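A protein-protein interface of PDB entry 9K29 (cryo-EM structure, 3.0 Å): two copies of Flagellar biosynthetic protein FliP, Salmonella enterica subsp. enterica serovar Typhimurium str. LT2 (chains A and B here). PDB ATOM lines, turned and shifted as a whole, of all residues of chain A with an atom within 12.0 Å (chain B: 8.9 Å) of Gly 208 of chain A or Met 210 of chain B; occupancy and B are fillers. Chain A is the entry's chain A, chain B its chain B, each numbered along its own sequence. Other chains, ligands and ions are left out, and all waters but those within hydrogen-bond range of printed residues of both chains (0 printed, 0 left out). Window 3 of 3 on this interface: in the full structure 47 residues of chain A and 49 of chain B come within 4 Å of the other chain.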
ATOM      1  N   VAL A 199     -13.985  -6.590 -12.488  1.00  0.00           N
ATOM      2  CA  VAL A 199     -13.402  -7.817 -11.949  1.00  0.00           C
ATOM      3  C   VAL A 199     -12.331  -7.486 -10.917  1.00  0.00           C
ATOM      4  O   VAL A 199     -12.299  -8.061  -9.820  1.00  0.00           O
ATOM      5  CB  VAL A 199     -12.840  -8.688 -13.086  1.00  0.00           C
ATOM      6  CG1 VAL A 199     -11.919  -9.759 -12.530  1.00  0.00           C
ATOM      7  CG2 VAL A 199     -13.974  -9.317 -13.874  1.00  0.00           C
ATOM      8  N   ILE A 200     -11.447  -6.543 -11.248  1.00  0.00           N
ATOM      9  CA  ILE A 200     -10.360  -6.196 -10.340  1.00  0.00           C
ATOM     10  C   ILE A 200     -10.902  -5.540  -9.079  1.00  0.00           C
ATOM     11  O   ILE A 200     -10.432  -5.820  -7.969  1.00  0.00           O
ATOM     12  CB  ILE A 200      -9.334  -5.305 -11.062  1.00  0.00           C
ATOM     13  CG1 ILE A 200      -8.456  -6.162 -11.972  1.00  0.00           C
ATOM     14  CG2 ILE A 200      -8.480  -4.542 -10.067  1.00  0.00           C
ATOM     15  CD1 ILE A 200      -7.543  -5.370 -12.860  1.00  0.00           C
ATOM     16  N   ALA A 201     -11.899  -4.662  -9.219  1.00  0.00           N
ATOM     17  CA  ALA A 201     -12.491  -4.033  -8.045  1.00  0.00           C
ATOM     18  C   ALA A 201     -13.144  -5.066  -7.138  1.00  0.00           C
ATOM     19  O   ALA A 201     -12.981  -5.017  -5.913  1.00  0.00           O
ATOM     20  CB  ALA A 201     -13.507  -2.973  -8.472  1.00  0.00           C
ATOM     21  N   SER A 202     -13.874  -6.019  -7.721  1.00  0.00           N
ATOM     22  CA  SER A 202     -14.511  -7.057  -6.918  1.00  0.00           C
ATOM     23  C   SER A 202     -13.476  -7.919  -6.205  1.00  0.00           C
ATOM     24  O   SER A 202     -13.643  -8.250  -5.027  1.00  0.00           O
ATOM     25  CB  SER A 202     -15.418  -7.918  -7.795  1.00  0.00           C
ATOM     26  OG  SER A 202     -14.796  -8.221  -9.029  1.00  0.00           O
ATOM     27  N   VAL A 203     -12.397  -8.289  -6.900  1.00  0.00           N
ATOM     28  CA  VAL A 203     -11.371  -9.123  -6.278  1.00  0.00           C
ATOM     29  C   VAL A 203     -10.685  -8.375  -5.141  1.00  0.00           C
ATOM     30  O   VAL A 203     -10.500  -8.916  -4.041  1.00  0.00           O
ATOM     31  CB  VAL A 203     -10.357  -9.600  -7.333  1.00  0.00           C
ATOM     32  CG1 VAL A 203      -9.131 -10.195  -6.661  1.00  0.00           C
ATOM     33  CG2 VAL A 203     -11.005 -10.610  -8.264  1.00  0.00           C
ATOM     34  N   LEU A 204     -10.316  -7.114  -5.380  1.00  0.00           N
ATOM     35  CA  LEU A 204      -9.667  -6.325  -4.341  1.00  0.00           C
ATOM     36  C   LEU A 204     -10.583  -6.145  -3.138  1.00  0.00           C
ATOM     37  O   LEU A 204     -10.133  -6.222  -1.989  1.00  0.00           O
ATOM     38  CB  LEU A 204      -9.243  -4.966  -4.901  1.00  0.00           C
ATOM     39  CG  LEU A 204      -8.012  -4.933  -5.808  1.00  0.00           C
ATOM     40  CD1 LEU A 204      -7.908  -3.591  -6.510  1.00  0.00           C
ATOM     41  CD2 LEU A 204      -6.748  -5.215  -5.018  1.00  0.00           C
ATOM     42  N   MET A 205     -11.875  -5.916  -3.381  1.00  0.00           N
ATOM     43  CA  MET A 205     -12.803  -5.731  -2.273  1.00  0.00           C
ATOM     44  C   MET A 205     -13.007  -7.028  -1.500  1.00  0.00           C
ATOM     45  O   MET A 205     -13.102  -7.014  -0.268  1.00  0.00           O
ATOM     46  CB  MET A 205     -14.138  -5.203  -2.787  1.00  0.00           C
ATOM     47  CG  MET A 205     -15.062  -4.844  -1.665  1.00  0.00           C
ATOM     48  SD  MET A 205     -14.344  -3.452  -0.779  1.00  0.00           S
ATOM     49  CE  MET A 205     -15.105  -3.635   0.822  1.00  0.00           C
ATOM     50  N   ALA A 206     -13.083  -8.156  -2.204  1.00  0.00           N
ATOM     51  CA  ALA A 206     -13.178  -9.457  -1.559  1.00  0.00           C
ATOM     52  C   ALA A 206     -11.925  -9.814  -0.780  1.00  0.00           C
ATOM     53  O   ALA A 206     -12.003 -10.626   0.148  1.00  0.00           O
ATOM     54  CB  ALA A 206     -13.466 -10.542  -2.597  1.00  0.00           C
ATOM     55  N   LEU A 207     -10.781  -9.229  -1.126  1.00  0.00           N
ATOM     56  CA  LEU A 207      -9.567  -9.394  -0.344  1.00  0.00           C
ATOM     57  C   LEU A 207      -9.494  -8.425   0.826  1.00  0.00           C
ATOM     58  O   LEU A 207      -8.486  -8.409   1.539  1.00  0.00           O
ATOM     59  CB  LEU A 207      -8.333  -9.225  -1.236  1.00  0.00           C
ATOM     60  CG  LEU A 207      -8.099 -10.367  -2.222  1.00  0.00           C
ATOM     61  CD1 LEU A 207      -6.897 -10.085  -3.106  1.00  0.00           C
ATOM     62  CD2 LEU A 207      -7.930 -11.675  -1.474  1.00  0.00           C
ATOM     63  N   GLY A 208     -10.531  -7.620   1.042  1.00  0.00           N
ATOM     64  CA  GLY A 208     -10.536  -6.677   2.143  1.00  0.00           C
ATOM     65  C   GLY A 208      -9.803  -5.386   1.860  1.00  0.00           C
ATOM     66  O   GLY A 208      -9.716  -4.526   2.741  1.00  0.00           O
ATOM     67  N   MET A 209      -9.281  -5.221   0.645  1.00  0.00           N
ATOM     68  CA  MET A 209      -8.509  -4.038   0.275  1.00  0.00           C
ATOM     69  C   MET A 209      -9.479  -2.942  -0.157  1.00  0.00           C
ATOM     70  O   MET A 209      -9.633  -2.633  -1.338  1.00  0.00           O
ATOM     71  CB  MET A 209      -7.507  -4.380  -0.820  1.00  0.00           C
ATOM     72  CG  MET A 209      -6.401  -5.319  -0.374  1.00  0.00           C
ATOM     73  SD  MET A 209      -5.242  -5.708  -1.696  1.00  0.00           S
ATOM     74  CE  MET A 209      -4.168  -6.876  -0.868  1.00  0.00           C
ATOM     75  N   MET A 210     -10.141  -2.342   0.834  1.00  0.00           N
ATOM     76  CA  MET A 210     -11.135  -1.314   0.555  1.00  0.00           C
ATOM     77  C   MET A 210     -10.504   0.013   0.151  1.00  0.00           C
ATOM     78  O   MET A 210     -11.095   0.757  -0.639  1.00  0.00           O
ATOM     79  CB  MET A 210     -12.033  -1.107   1.775  1.00  0.00           C
ATOM     80  CG  MET A 210     -11.295  -1.189   3.100  1.00  0.00           C
ATOM     81  SD  MET A 210     -12.403  -1.381   4.506  1.00  0.00           S
ATOM     82  CE  MET A 210     -13.118   0.257   4.585  1.00  0.00           C
ATOM     83  N   MET A 211      -9.320   0.328   0.675  1.00  0.00           N
ATOM     84  CA  MET A 211      -8.669   1.600   0.395  1.00  0.00           C
ATOM     85  C   MET A 211      -7.783   1.567  -0.843  1.00  0.00           C
ATOM     86  O   MET A 211      -7.326   2.627  -1.283  1.00  0.00           O
ATOM     87  CB  MET A 211      -7.830   2.042   1.601  1.00  0.00           C
ATOM     88  CG  MET A 211      -8.632   2.662   2.730  1.00  0.00           C
ATOM     89  SD  MET A 211      -9.601   4.082   2.193  1.00  0.00           S
ATOM     90  CE  MET A 211     -10.600   4.370   3.650  1.00  0.00           C
ATOM     91  N   VAL A 212      -7.532   0.396  -1.411  1.00  0.00           N
ATOM     92  CA  VAL A 212      -6.727   0.331  -2.635  1.00  0.00           C
ATOM     93  C   VAL A 212      -7.575   0.790  -3.814  1.00  0.00           C
ATOM     94  O   VAL A 212      -8.693   0.279  -4.003  1.00  0.00           O
ATOM     95  CB  VAL A 212      -6.198  -1.088  -2.851  1.00  0.00           C
ATOM     96  CG1 VAL A 212      -5.215  -1.114  -4.002  1.00  0.00           C
ATOM     97  CG2 VAL A 212      -5.534  -1.594  -1.585  1.00  0.00           C
ATOM     98  N   PRO A 213      -7.105   1.736  -4.622  1.00  0.00           N
ATOM     99  CA  PRO A 213      -7.907   2.214  -5.750  1.00  0.00           C
ATOM    100  C   PRO A 213      -7.794   1.270  -6.934  1.00  0.00           C
ATOM    101  O   PRO A 213      -6.689   1.012  -7.432  1.00  0.00           O
ATOM    102  CB  PRO A 213      -7.297   3.587  -6.063  1.00  0.00           C
ATOM    103  CG  PRO A 213      -5.902   3.528  -5.533  1.00  0.00           C
ATOM    104  CD  PRO A 213      -5.807   2.423  -4.517  1.00  0.00           C
ATOM    105  N   PRO A 214      -8.920   0.729  -7.405  1.00  0.00           N
ATOM    106  CA  PRO A 214      -8.860  -0.268  -8.487  1.00  0.00           C
ATOM    107  C   PRO A 214      -8.264   0.253  -9.782  1.00  0.00           C
ATOM    108  O   PRO A 214      -7.774  -0.549 -10.584  1.00  0.00           O
ATOM    109  CB  PRO A 214     -10.330  -0.669  -8.674  1.00  0.00           C
ATOM    110  CG  PRO A 214     -10.996  -0.308  -7.395  1.00  0.00           C
ATOM    111  CD  PRO A 214     -10.285   0.902  -6.883  1.00  0.00           C
ATOM    112  N   ILE A 217      -4.462  -0.471 -10.439  1.00  0.00           N
ATOM    113  CA  ILE A 217      -4.137  -1.854 -10.766  1.00  0.00           C
ATOM    114  C   ILE A 217      -4.765  -2.268 -12.095  1.00  0.00           C
ATOM    115  O   ILE A 217      -4.210  -3.108 -12.811  1.00  0.00           O
ATOM    116  CB  ILE A 217      -4.575  -2.787  -9.623  1.00  0.00           C
ATOM    117  CG1 ILE A 217      -3.757  -2.505  -8.362  1.00  0.00           C
ATOM    118  CG2 ILE A 217      -4.413  -4.249 -10.007  1.00  0.00           C
ATOM    119  CD1 ILE A 217      -4.419  -1.551  -7.409  1.00  0.00           C
ATOM    120  N   ALA B 201      -0.098  -3.120   0.119  1.00  0.00           N
ATOM    121  CA  ALA B 201      -1.494  -3.372   0.465  1.00  0.00           C
ATOM    122  C   ALA B 201      -1.648  -4.682   1.225  1.00  0.00           C
ATOM    123  O   ALA B 201      -2.387  -4.750   2.214  1.00  0.00           O
ATOM    124  CB  ALA B 201      -2.354  -3.378  -0.798  1.00  0.00           C
ATOM    125  N   VAL B 203       0.643  -6.222   3.050  1.00  0.00           N
ATOM    126  CA  VAL B 203       1.227  -6.070   4.380  1.00  0.00           C
ATOM    127  C   VAL B 203       0.279  -5.304   5.292  1.00  0.00           C
ATOM    128  O   VAL B 203       0.080  -5.673   6.458  1.00  0.00           O
ATOM    129  CB  VAL B 203       2.604  -5.387   4.285  1.00  0.00           C
ATOM    130  CG1 VAL B 203       3.072  -4.942   5.659  1.00  0.00           C
ATOM    131  CG2 VAL B 203       3.616  -6.329   3.659  1.00  0.00           C
ATOM    132  N   LEU B 204      -0.327  -4.231   4.778  1.00  0.00           N
ATOM    133  CA  LEU B 204      -1.277  -3.472   5.584  1.00  0.00           C
ATOM    134  C   LEU B 204      -2.473  -4.326   5.979  1.00  0.00           C
ATOM    135  O   LEU B 204      -2.909  -4.295   7.134  1.00  0.00           O
ATOM    136  CB  LEU B 204      -1.732  -2.223   4.830  1.00  0.00           C
ATOM    137  CG  LEU B 204      -0.684  -1.123   4.658  1.00  0.00           C
ATOM    138  CD1 LEU B 204      -1.232   0.013   3.813  1.00  0.00           C
ATOM    139  CD2 LEU B 204      -0.220  -0.611   6.011  1.00  0.00           C
ATOM    140  N   MET B 205      -3.007  -5.111   5.038  1.00  0.00           N
ATOM    141  CA  MET B 205      -4.136  -5.980   5.358  1.00  0.00           C
ATOM    142  C   MET B 205      -3.754  -7.026   6.397  1.00  0.00           C
ATOM    143  O   MET B 205      -4.549  -7.344   7.288  1.00  0.00           O
ATOM    144  CB  MET B 205      -4.665  -6.655   4.093  1.00  0.00           C
ATOM    145  CG  MET B 205      -5.271  -5.703   3.075  1.00  0.00           C
ATOM    146  SD  MET B 205      -6.702  -4.802   3.697  1.00  0.00           S
ATOM    147  CE  MET B 205      -5.978  -3.202   4.044  1.00  0.00           C
ATOM    148  N   ALA B 206      -2.543  -7.577   6.294  1.00  0.00           N
ATOM    149  CA  ALA B 206      -2.076  -8.520   7.304  1.00  0.00           C
ATOM    150  C   ALA B 206      -2.002  -7.858   8.671  1.00  0.00           C
ATOM    151  O   ALA B 206      -2.383  -8.457   9.683  1.00  0.00           O
ATOM    152  CB  ALA B 206      -0.715  -9.086   6.908  1.00  0.00           C
ATOM    153  N   LEU B 207      -1.518  -6.618   8.720  1.00  0.00           N
ATOM    154  CA  LEU B 207      -1.482  -5.860   9.963  1.00  0.00           C
ATOM    155  C   LEU B 207      -2.849  -5.339  10.382  1.00  0.00           C
ATOM    156  O   LEU B 207      -2.975  -4.799  11.486  1.00  0.00           O
ATOM    157  CB  LEU B 207      -0.509  -4.687   9.830  1.00  0.00           C
ATOM    158  CG  LEU B 207       0.972  -5.061   9.819  1.00  0.00           C
ATOM    159  CD1 LEU B 207       1.839  -3.825   9.658  1.00  0.00           C
ATOM    160  CD2 LEU B 207       1.325  -5.807  11.094  1.00  0.00           C
ATOM    161  N   GLY B 208      -3.867  -5.490   9.540  1.00  0.00           N
ATOM    162  CA  GLY B 208      -5.160  -4.886   9.790  1.00  0.00           C
ATOM    163  C   GLY B 208      -5.338  -3.648   8.938  1.00  0.00           C
ATOM    164  O   GLY B 208      -5.461  -3.751   7.714  1.00  0.00           O
ATOM    165  N   MET B 209      -5.376  -2.487   9.590  1.00  0.00           N
ATOM    166  CA  MET B 209      -5.271  -1.174   8.948  1.00  0.00           C
ATOM    167  C   MET B 209      -6.038  -1.046   7.635  1.00  0.00           C
ATOM    168  O   MET B 209      -5.560  -0.473   6.654  1.00  0.00           O
ATOM    169  CB  MET B 209      -3.806  -0.784   8.765  1.00  0.00           C
ATOM    170  CG  MET B 209      -2.939  -1.011   9.992  1.00  0.00           C
ATOM    171  SD  MET B 209      -1.314  -0.259   9.796  1.00  0.00           S
ATOM    172  CE  MET B 209      -0.894   0.099  11.495  1.00  0.00           C
ATOM    173  N   MET B 210      -7.253  -1.597   7.618  1.00  0.00           N
ATOM    174  CA  MET B 210      -8.113  -1.411   6.456  1.00  0.00           C
ATOM    175  C   MET B 210      -8.523   0.031   6.200  1.00  0.00           C
ATOM    176  O   MET B 210      -9.069   0.319   5.130  1.00  0.00           O
ATOM    177  CB  MET B 210      -9.352  -2.301   6.561  1.00  0.00           C
ATOM    178  CG  MET B 210      -9.024  -3.786   6.533  1.00  0.00           C
ATOM    179  SD  MET B 210     -10.469  -4.860   6.585  1.00  0.00           S
ATOM    180  CE  MET B 210     -10.962  -4.695   8.294  1.00  0.00           C
ATOM    181  N   MET B 211      -8.271   0.936   7.145  1.00  0.00           N
ATOM    182  CA  MET B 211      -8.555   2.350   6.964  1.00  0.00           C
ATOM    183  C   MET B 211      -7.394   3.116   6.349  1.00  0.00           C
ATOM    184  O   MET B 211      -7.607   4.210   5.818  1.00  0.00           O
ATOM    185  CB  MET B 211      -8.907   2.997   8.310  1.00  0.00           C
ATOM    186  CG  MET B 211     -10.132   2.415   9.001  1.00  0.00           C
ATOM    187  SD  MET B 211     -11.642   2.284   8.020  1.00  0.00           S
ATOM    188  CE  MET B 211     -11.644   3.856   7.166  1.00  0.00           C
ATOM    189  N   VAL B 212      -6.185   2.571   6.412  1.00  0.00           N
ATOM    190  CA  VAL B 212      -4.993   3.244   5.906  1.00  0.00           C
ATOM    191  C   VAL B 212      -4.934   3.102   4.390  1.00  0.00           C
ATOM    192  O   VAL B 212      -4.900   1.976   3.875  1.00  0.00           O
ATOM    193  CB  VAL B 212      -3.722   2.683   6.559  1.00  0.00           C
ATOM    194  CG1 VAL B 212      -2.510   3.461   6.098  1.00  0.00           C
ATOM    195  CG2 VAL B 212      -3.846   2.735   8.070  1.00  0.00           C
ATOM    196  N   PRO B 213      -4.922   4.200   3.641  1.00  0.00           N
ATOM    197  CA  PRO B 213      -4.756   4.104   2.192  1.00  0.00           C
ATOM    198  C   PRO B 213      -3.328   3.731   1.838  1.00  0.00           C
ATOM    199  O   PRO B 213      -2.378   4.409   2.255  1.00  0.00           O
ATOM    200  CB  PRO B 213      -5.106   5.516   1.699  1.00  0.00           C
ATOM    201  CG  PRO B 213      -4.851   6.399   2.861  1.00  0.00           C
ATOM    202  CD  PRO B 213      -5.112   5.588   4.095  1.00  0.00           C
ATOM    203  N   PRO B 214      -3.135   2.654   1.074  1.00  0.00           N
ATOM    204  CA  PRO B 214      -1.767   2.218   0.753  1.00  0.00           C
ATOM    205  C   PRO B 214      -0.994   3.198  -0.108  1.00  0.00           C
ATOM    206  O   PRO B 214       0.234   3.091  -0.180  1.00  0.00           O
ATOM    207  CB  PRO B 214      -1.986   0.888   0.022  1.00  0.00           C
ATOM    208  CG  PRO B 214      -3.351   1.004  -0.550  1.00  0.00           C
ATOM    209  CD  PRO B 214      -4.150   1.795   0.443  1.00  0.00           C
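The backbone carbonyl oxygen of Gly 208 of chain A lies close to the side-chain sulfur of Met 205 of chain B (3.2 Å). SD of Met 210 of chain A sits close to O of Met 210 of chain B (3.8 Å).
The backbone NH (N) of Met 209 of chain A sits at hydrogen-bond distance from the backbone carbonyl oxygen (O) of Leu 204 of chain A, 2.9 Å away.
CG of Met 210 of chain B touches O of Gly 208 of chain A, at 3.9 Å. SD of Met 209 of chain A touches CB of Ala 201 of chain B, at 3.8 Å. Met 209 of chain A touches Met 205 of chain B. Met 210 of chain B touches Met 211 of chain A (O to CG, 3.4 Å). CG of Met 211 of chain A touches O of Met 211 of chain B (3.6 Å). O of Val 212 of chain B touches CB of Met 211 of chain A (3.7 Å). Met 211 of chain A touches Pro 213 of chain B. Met 211 of chain A touches Pro 214 of chain B (O to CD, 3.7 Å). CG2 of Val 212 of chain A touches CB of Ala 201 of chain B, 3.7 Å away. Val 212 of chain A touches Pro 214 of chain B (CG2 to CG, 3.5 Å).
Of the printed residues of chain B, Gly 208 of chain A touches Met 205 and Met 210. Printed residues of chain B within 4 Å of Met 210 of chain A: Met 210. Of the printed residues of chain B, Met 211 of chain A touches Met 210, Met 211, Val 212, Pro 213 and Pro 214. Pro 214 of chain A touches none of the printed residues of chain B. Of chain A, only Gly 208 (3.2 Å) and Met 209 (3.6 Å) come within 4 Å of Met 205 of chain B. No residue of chain A comes within 4 Å of Gly 208 of chain B. Met 210 of chain B touches three residues of chain A. Printed residues of chain A within 4 Å of Met 211 of chain B: Met 211 (3.6 Å). The nearest residue of chain A that does not touch Met 210 of chain B is Met 209 of chain A (6.1 Å). The nearest printed residue of chain A that does not touch Pro 214 of chain B is Pro 213 of chain A (4.9 Å).
Of the 17 printed residues of chain A, 5 touch a printed residue of chain B.
Met 209 of chain A touches Ala 201 of chain B, but with the chains exchanged Ala 201 of chain A does not touch Met 209 of chain B (15.3 Å). Met 211 of chain A touches its own counterpart, Met 211 of chain B. Met 211 of chain A touches Val 212 of chain B, but with the chains exchanged Val 212 of chain A does not touch Met 211 of chain B (8.2 Å). Met 211 of chain A touches Pro 214 of chain B, but with the chains exchanged Pro 214 of chain A does not touch Met 211 of chain B (13.4 Å). Positions printed for both chains: 201, 203, 204, 205, 206, 207, 208, 209, 210, 211, 212, 213 and 214. Of the 12 pairs that touch across the chains among the printed residues, 2 have their exchanged pair printed and touching as well.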
